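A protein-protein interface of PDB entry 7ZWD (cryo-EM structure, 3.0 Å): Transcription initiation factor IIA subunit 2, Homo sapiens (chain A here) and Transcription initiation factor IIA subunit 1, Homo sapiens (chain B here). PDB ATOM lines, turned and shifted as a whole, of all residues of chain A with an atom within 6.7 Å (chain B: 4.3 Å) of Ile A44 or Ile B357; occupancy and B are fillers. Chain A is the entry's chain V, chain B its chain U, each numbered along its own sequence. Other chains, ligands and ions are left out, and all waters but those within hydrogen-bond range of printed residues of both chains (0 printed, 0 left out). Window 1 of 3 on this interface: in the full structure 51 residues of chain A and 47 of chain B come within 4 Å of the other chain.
Hydrophobic or aromatic side chains of chain A that line the printed part of chain B: Tyr A6, Leu A11, Ile A44 and Leu A48.
Along chain A the printed residues that touch a printed residue of chain B span positions 6 to 48.
Among the printed residues, 7 pairs touch across the chains.
Among the printed residues, no Asp or Glu carboxylate lies within 4 Å of a Lys or Arg side-chain nitrogen of the other chain.
Tyr A6 touches Val B336 (CE1 to O, 3.6 Å).
Ile B357 touches Tyr A6 (CD1 to CD1, 3.9 Å).
Thr A10 touches Tyr B14 (OG1 to OH, 3.8 Å).
Leu A11 touches Tyr B14.
Ile B357 touches Ile A44.
Leu A48 touches Ile B357.
CG2 of Ile B366 touches CD2 of Leu A48, at 3.7 Å.
O of Val B336 sits at hydrogen-bond distance from N of Ile B357, 3.0 Å away.
The backbone carbonyl oxygen of Tyr A6 is in hydrogen-bond range of the side-chain hydroxyl of Thr A9 (2.9 Å).
Of the printed residues of chain B, Thr A10 touches Tyr B14 (3.8 Å).
Ile A44 touches one residue of chain B.
Ala A47 touches none of the printed residues of chain B.
Of the printed residues of chain B, Leu A48 touches Ile B357 (3.7 Å) and Ile B366 (3.7 Å).
Printed residues of chain A within 4 Å of Tyr B14: Thr A10 (3.8 Å) and Leu A11 (3.7 Å).
Of chain A, only Tyr A6 (3.9 Å), Ile A44 (3.7 Å) and Leu A48 (3.7 Å) come within 4 Å of Ile B357.
The nearest printed residue of chain B that does not touch Ile A44 is Tyr B14 (5.7 Å).
The nearest residue of chain A that does not touch Ile B357 is Thr A9 (4.1 Å).
The nearest printed residue of chain B that does not touch Thr A10 is Ile B357 (6.1 Å).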
ATOM      1  N   TYR A   6      22.000   1.371  26.107  1.00  0.00           N
ATOM      2  CA  TYR A   6      21.113   2.296  26.787  1.00  0.00           C
ATOM      3  C   TYR A   6      21.854   3.358  27.570  1.00  0.00           C
ATOM      4  O   TYR A   6      21.209   4.195  28.202  1.00  0.00           O
ATOM      5  CB  TYR A   6      20.176   1.525  27.708  1.00  0.00           C
ATOM      6  CG  TYR A   6      19.230   0.630  26.959  1.00  0.00           C
ATOM      7  CD1 TYR A   6      18.063   1.127  26.420  1.00  0.00           C
ATOM      8  CD2 TYR A   6      19.507  -0.710  26.782  1.00  0.00           C
ATOM      9  CE1 TYR A   6      17.199   0.317  25.733  1.00  0.00           C
ATOM     10  CE2 TYR A   6      18.643  -1.526  26.096  1.00  0.00           C
ATOM     11  CZ  TYR A   6      17.492  -1.005  25.575  1.00  0.00           C
ATOM     12  OH  TYR A   6      16.622  -1.810  24.888  1.00  0.00           O
ATOM     13  N   ARG A   7      23.180   3.353  27.542  1.00  0.00           N
ATOM     14  CA  ARG A   7      23.959   4.401  28.195  1.00  0.00           C
ATOM     15  C   ARG A   7      24.230   5.538  27.219  1.00  0.00           C
ATOM     16  O   ARG A   7      25.349   6.015  27.061  1.00  0.00           O
ATOM     17  CB  ARG A   7      25.260   3.829  28.740  1.00  0.00           C
ATOM     18  CG  ARG A   7      25.071   2.887  29.891  1.00  0.00           C
ATOM     19  CD  ARG A   7      26.334   2.110  30.169  1.00  0.00           C
ATOM     20  NE  ARG A   7      27.516   2.943  30.014  1.00  0.00           N
ATOM     21  CZ  ARG A   7      28.755   2.507  30.196  1.00  0.00           C
ATOM     22  NH1 ARG A   7      28.965   1.248  30.548  1.00  0.00           N
ATOM     23  NH2 ARG A   7      29.780   3.330  30.032  1.00  0.00           N
ATOM     24  N   THR A   9      20.935   7.308  26.458  1.00  0.00           N
ATOM     25  CA  THR A   9      19.657   7.946  26.707  1.00  0.00           C
ATOM     26  C   THR A   9      19.794   8.985  27.809  1.00  0.00           C
ATOM     27  O   THR A   9      20.832   9.097  28.463  1.00  0.00           O
ATOM     28  CB  THR A   9      18.615   6.911  27.100  1.00  0.00           C
ATOM     29  OG1 THR A   9      19.064   6.210  28.264  1.00  0.00           O
ATOM     30  CG2 THR A   9      18.423   5.923  25.976  1.00  0.00           C
ATOM     31  N   THR A  10      18.722   9.750  28.011  1.00  0.00           N
ATOM     32  CA  THR A  10      18.742  10.777  29.046  1.00  0.00           C
ATOM     33  C   THR A  10      18.981  10.172  30.419  1.00  0.00           C
ATOM     34  O   THR A  10      19.692  10.754  31.244  1.00  0.00           O
ATOM     35  CB  THR A  10      17.439  11.568  29.033  1.00  0.00           C
ATOM     36  OG1 THR A  10      16.384  10.750  29.550  1.00  0.00           O
ATOM     37  CG2 THR A  10      17.106  12.014  27.622  1.00  0.00           C
ATOM     38  N   LEU A  11      18.411   8.998  30.679  1.00  0.00           N
ATOM     39  CA  LEU A  11      18.665   8.327  31.947  1.00  0.00           C
ATOM     40  C   LEU A  11      20.136   7.962  32.090  1.00  0.00           C
ATOM     41  O   LEU A  11      20.779   8.298  33.091  1.00  0.00           O
ATOM     42  CB  LEU A  11      17.790   7.086  32.061  1.00  0.00           C
ATOM     43  CG  LEU A  11      17.853   6.414  33.425  1.00  0.00           C
ATOM     44  CD1 LEU A  11      17.704   7.452  34.508  1.00  0.00           C
ATOM     45  CD2 LEU A  11      16.767   5.374  33.532  1.00  0.00           C
ATOM     46  N   GLY A  12      20.688   7.277  31.089  1.00  0.00           N
ATOM     47  CA  GLY A  12      22.081   6.878  31.165  1.00  0.00           C
ATOM     48  C   GLY A  12      23.030   8.058  31.129  1.00  0.00           C
ATOM     49  O   GLY A  12      24.062   8.055  31.800  1.00  0.00           O
ATOM     50  N   GLN A  39      25.644  -2.510  36.672  1.00  0.00           N
ATOM     51  CA  GLN A  39      24.393  -2.810  37.350  1.00  0.00           C
ATOM     52  C   GLN A  39      23.244  -2.026  36.745  1.00  0.00           C
ATOM     53  O   GLN A  39      22.134  -2.547  36.629  1.00  0.00           O
ATOM     54  CB  GLN A  39      24.517  -2.494  38.837  1.00  0.00           C
ATOM     55  CG  GLN A  39      23.210  -2.599  39.591  1.00  0.00           C
ATOM     56  CD  GLN A  39      22.554  -3.956  39.435  1.00  0.00           C
ATOM     57  OE1 GLN A  39      23.224  -4.988  39.456  1.00  0.00           O
ATOM     58  NE2 GLN A  39      21.237  -3.963  39.283  1.00  0.00           N
ATOM     59  N   PHE A  40      23.496  -0.787  36.331  1.00  0.00           N
ATOM     60  CA  PHE A  40      22.448   0.008  35.708  1.00  0.00           C
ATOM     61  C   PHE A  40      22.010  -0.602  34.393  1.00  0.00           C
ATOM     62  O   PHE A  40      20.822  -0.601  34.071  1.00  0.00           O
ATOM     63  CB  PHE A  40      22.924   1.439  35.481  1.00  0.00           C
ATOM     64  CG  PHE A  40      22.249   2.117  34.329  1.00  0.00           C
ATOM     65  CD1 PHE A  40      21.006   2.691  34.483  1.00  0.00           C
ATOM     66  CD2 PHE A  40      22.850   2.173  33.090  1.00  0.00           C
ATOM     67  CE1 PHE A  40      20.383   3.308  33.428  1.00  0.00           C
ATOM     68  CE2 PHE A  40      22.227   2.785  32.038  1.00  0.00           C
ATOM     69  CZ  PHE A  40      20.994   3.355  32.206  1.00  0.00           C
ATOM     70  N   ASP A  41      22.960  -1.087  33.599  1.00  0.00           N
ATOM     71  CA  ASP A  41      22.597  -1.716  32.335  1.00  0.00           C
ATOM     72  C   ASP A  41      21.716  -2.929  32.573  1.00  0.00           C
ATOM     73  O   ASP A  41      20.670  -3.096  31.928  1.00  0.00           O
ATOM     74  CB  ASP A  41      23.851  -2.097  31.559  1.00  0.00           C
ATOM     75  CG  ASP A  41      24.606  -0.893  31.072  1.00  0.00           C
ATOM     76  OD1 ASP A  41      23.962   0.162  30.919  1.00  0.00           O
ATOM     77  OD2 ASP A  41      25.829  -0.992  30.843  1.00  0.00           O
ATOM     78  N   LYS A  42      22.113  -3.780  33.519  1.00  0.00           N
ATOM     79  CA  LYS A  42      21.283  -4.937  33.840  1.00  0.00           C
ATOM     80  C   LYS A  42      19.906  -4.507  34.331  1.00  0.00           C
ATOM     81  O   LYS A  42      18.884  -5.083  33.935  1.00  0.00           O
ATOM     82  CB  LYS A  42      21.975  -5.806  34.885  1.00  0.00           C
ATOM     83  CG  LYS A  42      21.126  -6.957  35.385  1.00  0.00           C
ATOM     84  CD  LYS A  42      21.969  -7.986  36.120  1.00  0.00           C
ATOM     85  CE  LYS A  42      22.803  -7.336  37.208  1.00  0.00           C
ATOM     86  NZ  LYS A  42      23.763  -8.291  37.826  1.00  0.00           N
ATOM     87  N   ALA A  43      19.860  -3.477  35.175  1.00  0.00           N
ATOM     88  CA  ALA A  43      18.596  -3.037  35.748  1.00  0.00           C
ATOM     89  C   ALA A  43      17.671  -2.474  34.685  1.00  0.00           C
ATOM     90  O   ALA A  43      16.471  -2.758  34.693  1.00  0.00           O
ATOM     91  CB  ALA A  43      18.844  -1.995  36.833  1.00  0.00           C
ATOM     92  N   ILE A  44      18.202  -1.677  33.762  1.00  0.00           N
ATOM     93  CA  ILE A  44      17.330  -1.080  32.761  1.00  0.00           C
ATOM     94  C   ILE A  44      16.880  -2.122  31.760  1.00  0.00           C
ATOM     95  O   ILE A  44      15.759  -2.048  31.251  1.00  0.00           O
ATOM     96  CB  ILE A  44      18.001   0.111  32.065  1.00  0.00           C
ATOM     97  CG1 ILE A  44      16.944   0.947  31.365  1.00  0.00           C
ATOM     98  CG2 ILE A  44      18.996  -0.352  31.044  1.00  0.00           C
ATOM     99  CD1 ILE A  44      17.444   2.280  30.931  1.00  0.00           C
ATOM    100  N   ASN A  45      17.710  -3.124  31.471  1.00  0.00           N
ATOM    101  CA  ASN A  45      17.233  -4.203  30.618  1.00  0.00           C
ATOM    102  C   ASN A  45      16.087  -4.944  31.286  1.00  0.00           C
ATOM    103  O   ASN A  45      15.046  -5.191  30.666  1.00  0.00           O
ATOM    104  CB  ASN A  45      18.374  -5.154  30.285  1.00  0.00           C
ATOM    105  CG  ASN A  45      19.322  -4.571  29.278  1.00  0.00           C
ATOM    106  OD1 ASN A  45      18.998  -4.463  28.099  1.00  0.00           O
ATOM    107  ND2 ASN A  45      20.501  -4.176  29.736  1.00  0.00           N
ATOM    108  N   ALA A  46      16.247  -5.282  32.568  1.00  0.00           N
ATOM    109  CA  ALA A  46      15.184  -5.986  33.276  1.00  0.00           C
ATOM    110  C   ALA A  46      13.919  -5.143  33.356  1.00  0.00           C
ATOM    111  O   ALA A  46      12.806  -5.663  33.219  1.00  0.00           O
ATOM    112  CB  ALA A  46      15.654  -6.375  34.675  1.00  0.00           C
ATOM    113  N   ALA A  47      14.070  -3.837  33.567  1.00  0.00           N
ATOM    114  CA  ALA A  47      12.912  -2.956  33.639  1.00  0.00           C
ATOM    115  C   ALA A  47      12.185  -2.908  32.308  1.00  0.00           C
ATOM    116  O   ALA A  47      11.003  -3.250  32.222  1.00  0.00           O
ATOM    117  CB  ALA A  47      13.343  -1.556  34.061  1.00  0.00           C
ATOM    118  N   LEU A  48      12.884  -2.502  31.249  1.00  0.00           N
ATOM    119  CA  LEU A  48      12.252  -2.409  29.942  1.00  0.00           C
ATOM    120  C   LEU A  48      11.702  -3.741  29.466  1.00  0.00           C
ATOM    121  O   LEU A  48      10.804  -3.757  28.624  1.00  0.00           O
ATOM    122  CB  LEU A  48      13.241  -1.869  28.923  1.00  0.00           C
ATOM    123  CG  LEU A  48      13.633  -0.414  29.121  1.00  0.00           C
ATOM    124  CD1 LEU A  48      14.958  -0.153  28.474  1.00  0.00           C
ATOM    125  CD2 LEU A  48      12.582   0.468  28.525  1.00  0.00           C
ATOM    126  N   ALA A  49      12.214  -4.859  29.976  1.00  0.00           N
ATOM    127  CA  ALA A  49      11.646  -6.138  29.579  1.00  0.00           C
ATOM    128  C   ALA A  49      10.410  -6.486  30.384  1.00  0.00           C
ATOM    129  O   ALA A  49       9.468  -7.071  29.841  1.00  0.00           O
ATOM    130  CB  ALA A  49      12.687  -7.245  29.722  1.00  0.00           C
ATOM    131  N   TYR B  14      11.438   5.430  35.005  1.00  0.00           N
ATOM    132  CA  TYR B  14      12.741   5.957  35.381  1.00  0.00           C
ATOM    133  C   TYR B  14      12.939   5.900  36.885  1.00  0.00           C
ATOM    134  O   TYR B  14      14.029   5.576  37.362  1.00  0.00           O
ATOM    135  CB  TYR B  14      12.894   7.389  34.888  1.00  0.00           C
ATOM    136  CG  TYR B  14      13.177   7.501  33.420  1.00  0.00           C
ATOM    137  CD1 TYR B  14      13.323   8.737  32.822  1.00  0.00           C
ATOM    138  CD2 TYR B  14      13.296   6.376  32.631  1.00  0.00           C
ATOM    139  CE1 TYR B  14      13.581   8.849  31.480  1.00  0.00           C
ATOM    140  CE2 TYR B  14      13.555   6.477  31.288  1.00  0.00           C
ATOM    141  CZ  TYR B  14      13.695   7.716  30.717  1.00  0.00           C
ATOM    142  OH  TYR B  14      13.953   7.827  29.376  1.00  0.00           O
ATOM    143  N   VAL B 334      16.261  10.092  18.560  1.00  0.00           N
ATOM    144  CA  VAL B 334      16.970   8.823  18.528  1.00  0.00           C
ATOM    145  C   VAL B 334      16.144   7.779  19.257  1.00  0.00           C
ATOM    146  O   VAL B 334      15.536   8.069  20.290  1.00  0.00           O
ATOM    147  CB  VAL B 334      18.376   8.953  19.144  1.00  0.00           C
ATOM    148  CG1 VAL B 334      18.291   9.390  20.582  1.00  0.00           C
ATOM    149  CG2 VAL B 334      19.108   7.644  19.052  1.00  0.00           C
ATOM    150  N   VAL B 335      16.104   6.571  18.710  1.00  0.00           N
ATOM    151  CA  VAL B 335      15.379   5.457  19.306  1.00  0.00           C
ATOM    152  C   VAL B 335      16.383   4.356  19.579  1.00  0.00           C
ATOM    153  O   VAL B 335      16.875   3.711  18.648  1.00  0.00           O
ATOM    154  CB  VAL B 335      14.255   4.947  18.404  1.00  0.00           C
ATOM    155  CG1 VAL B 335      13.448   3.913  19.129  1.00  0.00           C
ATOM    156  CG2 VAL B 335      13.380   6.080  17.974  1.00  0.00           C
ATOM    157  N   VAL B 336      16.685   4.134  20.845  1.00  0.00           N
ATOM    158  CA  VAL B 336      17.628   3.110  21.263  1.00  0.00           C
ATOM    159  C   VAL B 336      16.817   1.900  21.699  1.00  0.00           C
ATOM    160  O   VAL B 336      16.115   1.946  22.712  1.00  0.00           O
ATOM    161  CB  VAL B 336      18.534   3.617  22.386  1.00  0.00           C
ATOM    162  CG1 VAL B 336      19.169   2.468  23.095  1.00  0.00           C
ATOM    163  CG2 VAL B 336      19.589   4.533  21.819  1.00  0.00           C
ATOM    164  N   GLY B 356      12.545  -0.472  24.180  1.00  0.00           N
ATOM    165  CA  GLY B 356      13.151   0.688  23.558  1.00  0.00           C
ATOM    166  C   GLY B 356      12.801   1.968  24.271  1.00  0.00           C
ATOM    167  O   GLY B 356      11.723   2.104  24.855  1.00  0.00           O
ATOM    168  N   ILE B 357      13.728   2.917  24.206  1.00  0.00           N
ATOM    169  CA  ILE B 357      13.574   4.251  24.760  1.00  0.00           C
ATOM    170  C   ILE B 357      13.835   5.241  23.643  1.00  0.00           C
ATOM    171  O   ILE B 357      14.974   5.380  23.191  1.00  0.00           O
ATOM    172  CB  ILE B 357      14.553   4.504  25.918  1.00  0.00           C
ATOM    173  CG1 ILE B 357      14.455   3.389  26.947  1.00  0.00           C
ATOM    174  CG2 ILE B 357      14.283   5.839  26.551  1.00  0.00           C
ATOM    175  CD1 ILE B 357      15.463   3.506  28.042  1.00  0.00           C
ATOM    176  N   MET B 358      12.799   5.937  23.204  1.00  0.00           N
ATOM    177  CA  MET B 358      12.945   6.902  22.131  1.00  0.00           C
ATOM    178  C   MET B 358      12.917   8.311  22.694  1.00  0.00           C
ATOM    179  O   MET B 358      12.382   8.550  23.774  1.00  0.00           O
ATOM    180  CB  MET B 358      11.860   6.728  21.079  1.00  0.00           C
ATOM    181  CG  MET B 358      10.501   6.414  21.623  1.00  0.00           C
ATOM    182  SD  MET B 358       9.481   5.688  20.340  1.00  0.00           S
ATOM    183  CE  MET B 358       7.944   5.470  21.215  1.00  0.00           C
ATOM    184  N   TYR B 365       9.953   8.606  25.301  1.00  0.00           N
ATOM    185  CA  TYR B 365       8.887   7.627  25.321  1.00  0.00           C
ATOM    186  C   TYR B 365       9.485   6.242  25.480  1.00  0.00           C
ATOM    187  O   TYR B 365      10.636   5.995  25.128  1.00  0.00           O
ATOM    188  CB  TYR B 365       8.051   7.686  24.051  1.00  0.00           C
ATOM    189  CG  TYR B 365       7.461   9.038  23.800  1.00  0.00           C
ATOM    190  CD1 TYR B 365       6.215   9.370  24.295  1.00  0.00           C
ATOM    191  CD2 TYR B 365       8.151   9.987  23.076  1.00  0.00           C
ATOM    192  CE1 TYR B 365       5.674  10.606  24.070  1.00  0.00           C
ATOM    193  CE2 TYR B 365       7.618  11.223  22.847  1.00  0.00           C
ATOM    194  CZ  TYR B 365       6.378  11.530  23.346  1.00  0.00           C
ATOM    195  OH  TYR B 365       5.841  12.770  23.117  1.00  0.00           O
ATOM    196  N   ILE B 366       8.679   5.340  26.015  1.00  0.00           N
ATOM    197  CA  ILE B 366       9.090   3.976  26.303  1.00  0.00           C
ATOM    198  C   ILE B 366       8.190   3.042  25.519  1.00  0.00           C
ATOM    199  O   ILE B 366       6.977   3.262  25.446  1.00  0.00           O
ATOM    200  CB  ILE B 366       8.995   3.676  27.810  1.00  0.00           C
ATOM    201  CG1 ILE B 366       9.849   4.652  28.602  1.00  0.00           C
ATOM    202  CG2 ILE B 366       9.437   2.287  28.094  1.00  0.00           C
ATOM    203  CD1 ILE B 366      11.306   4.490  28.355  1.00  0.00           C
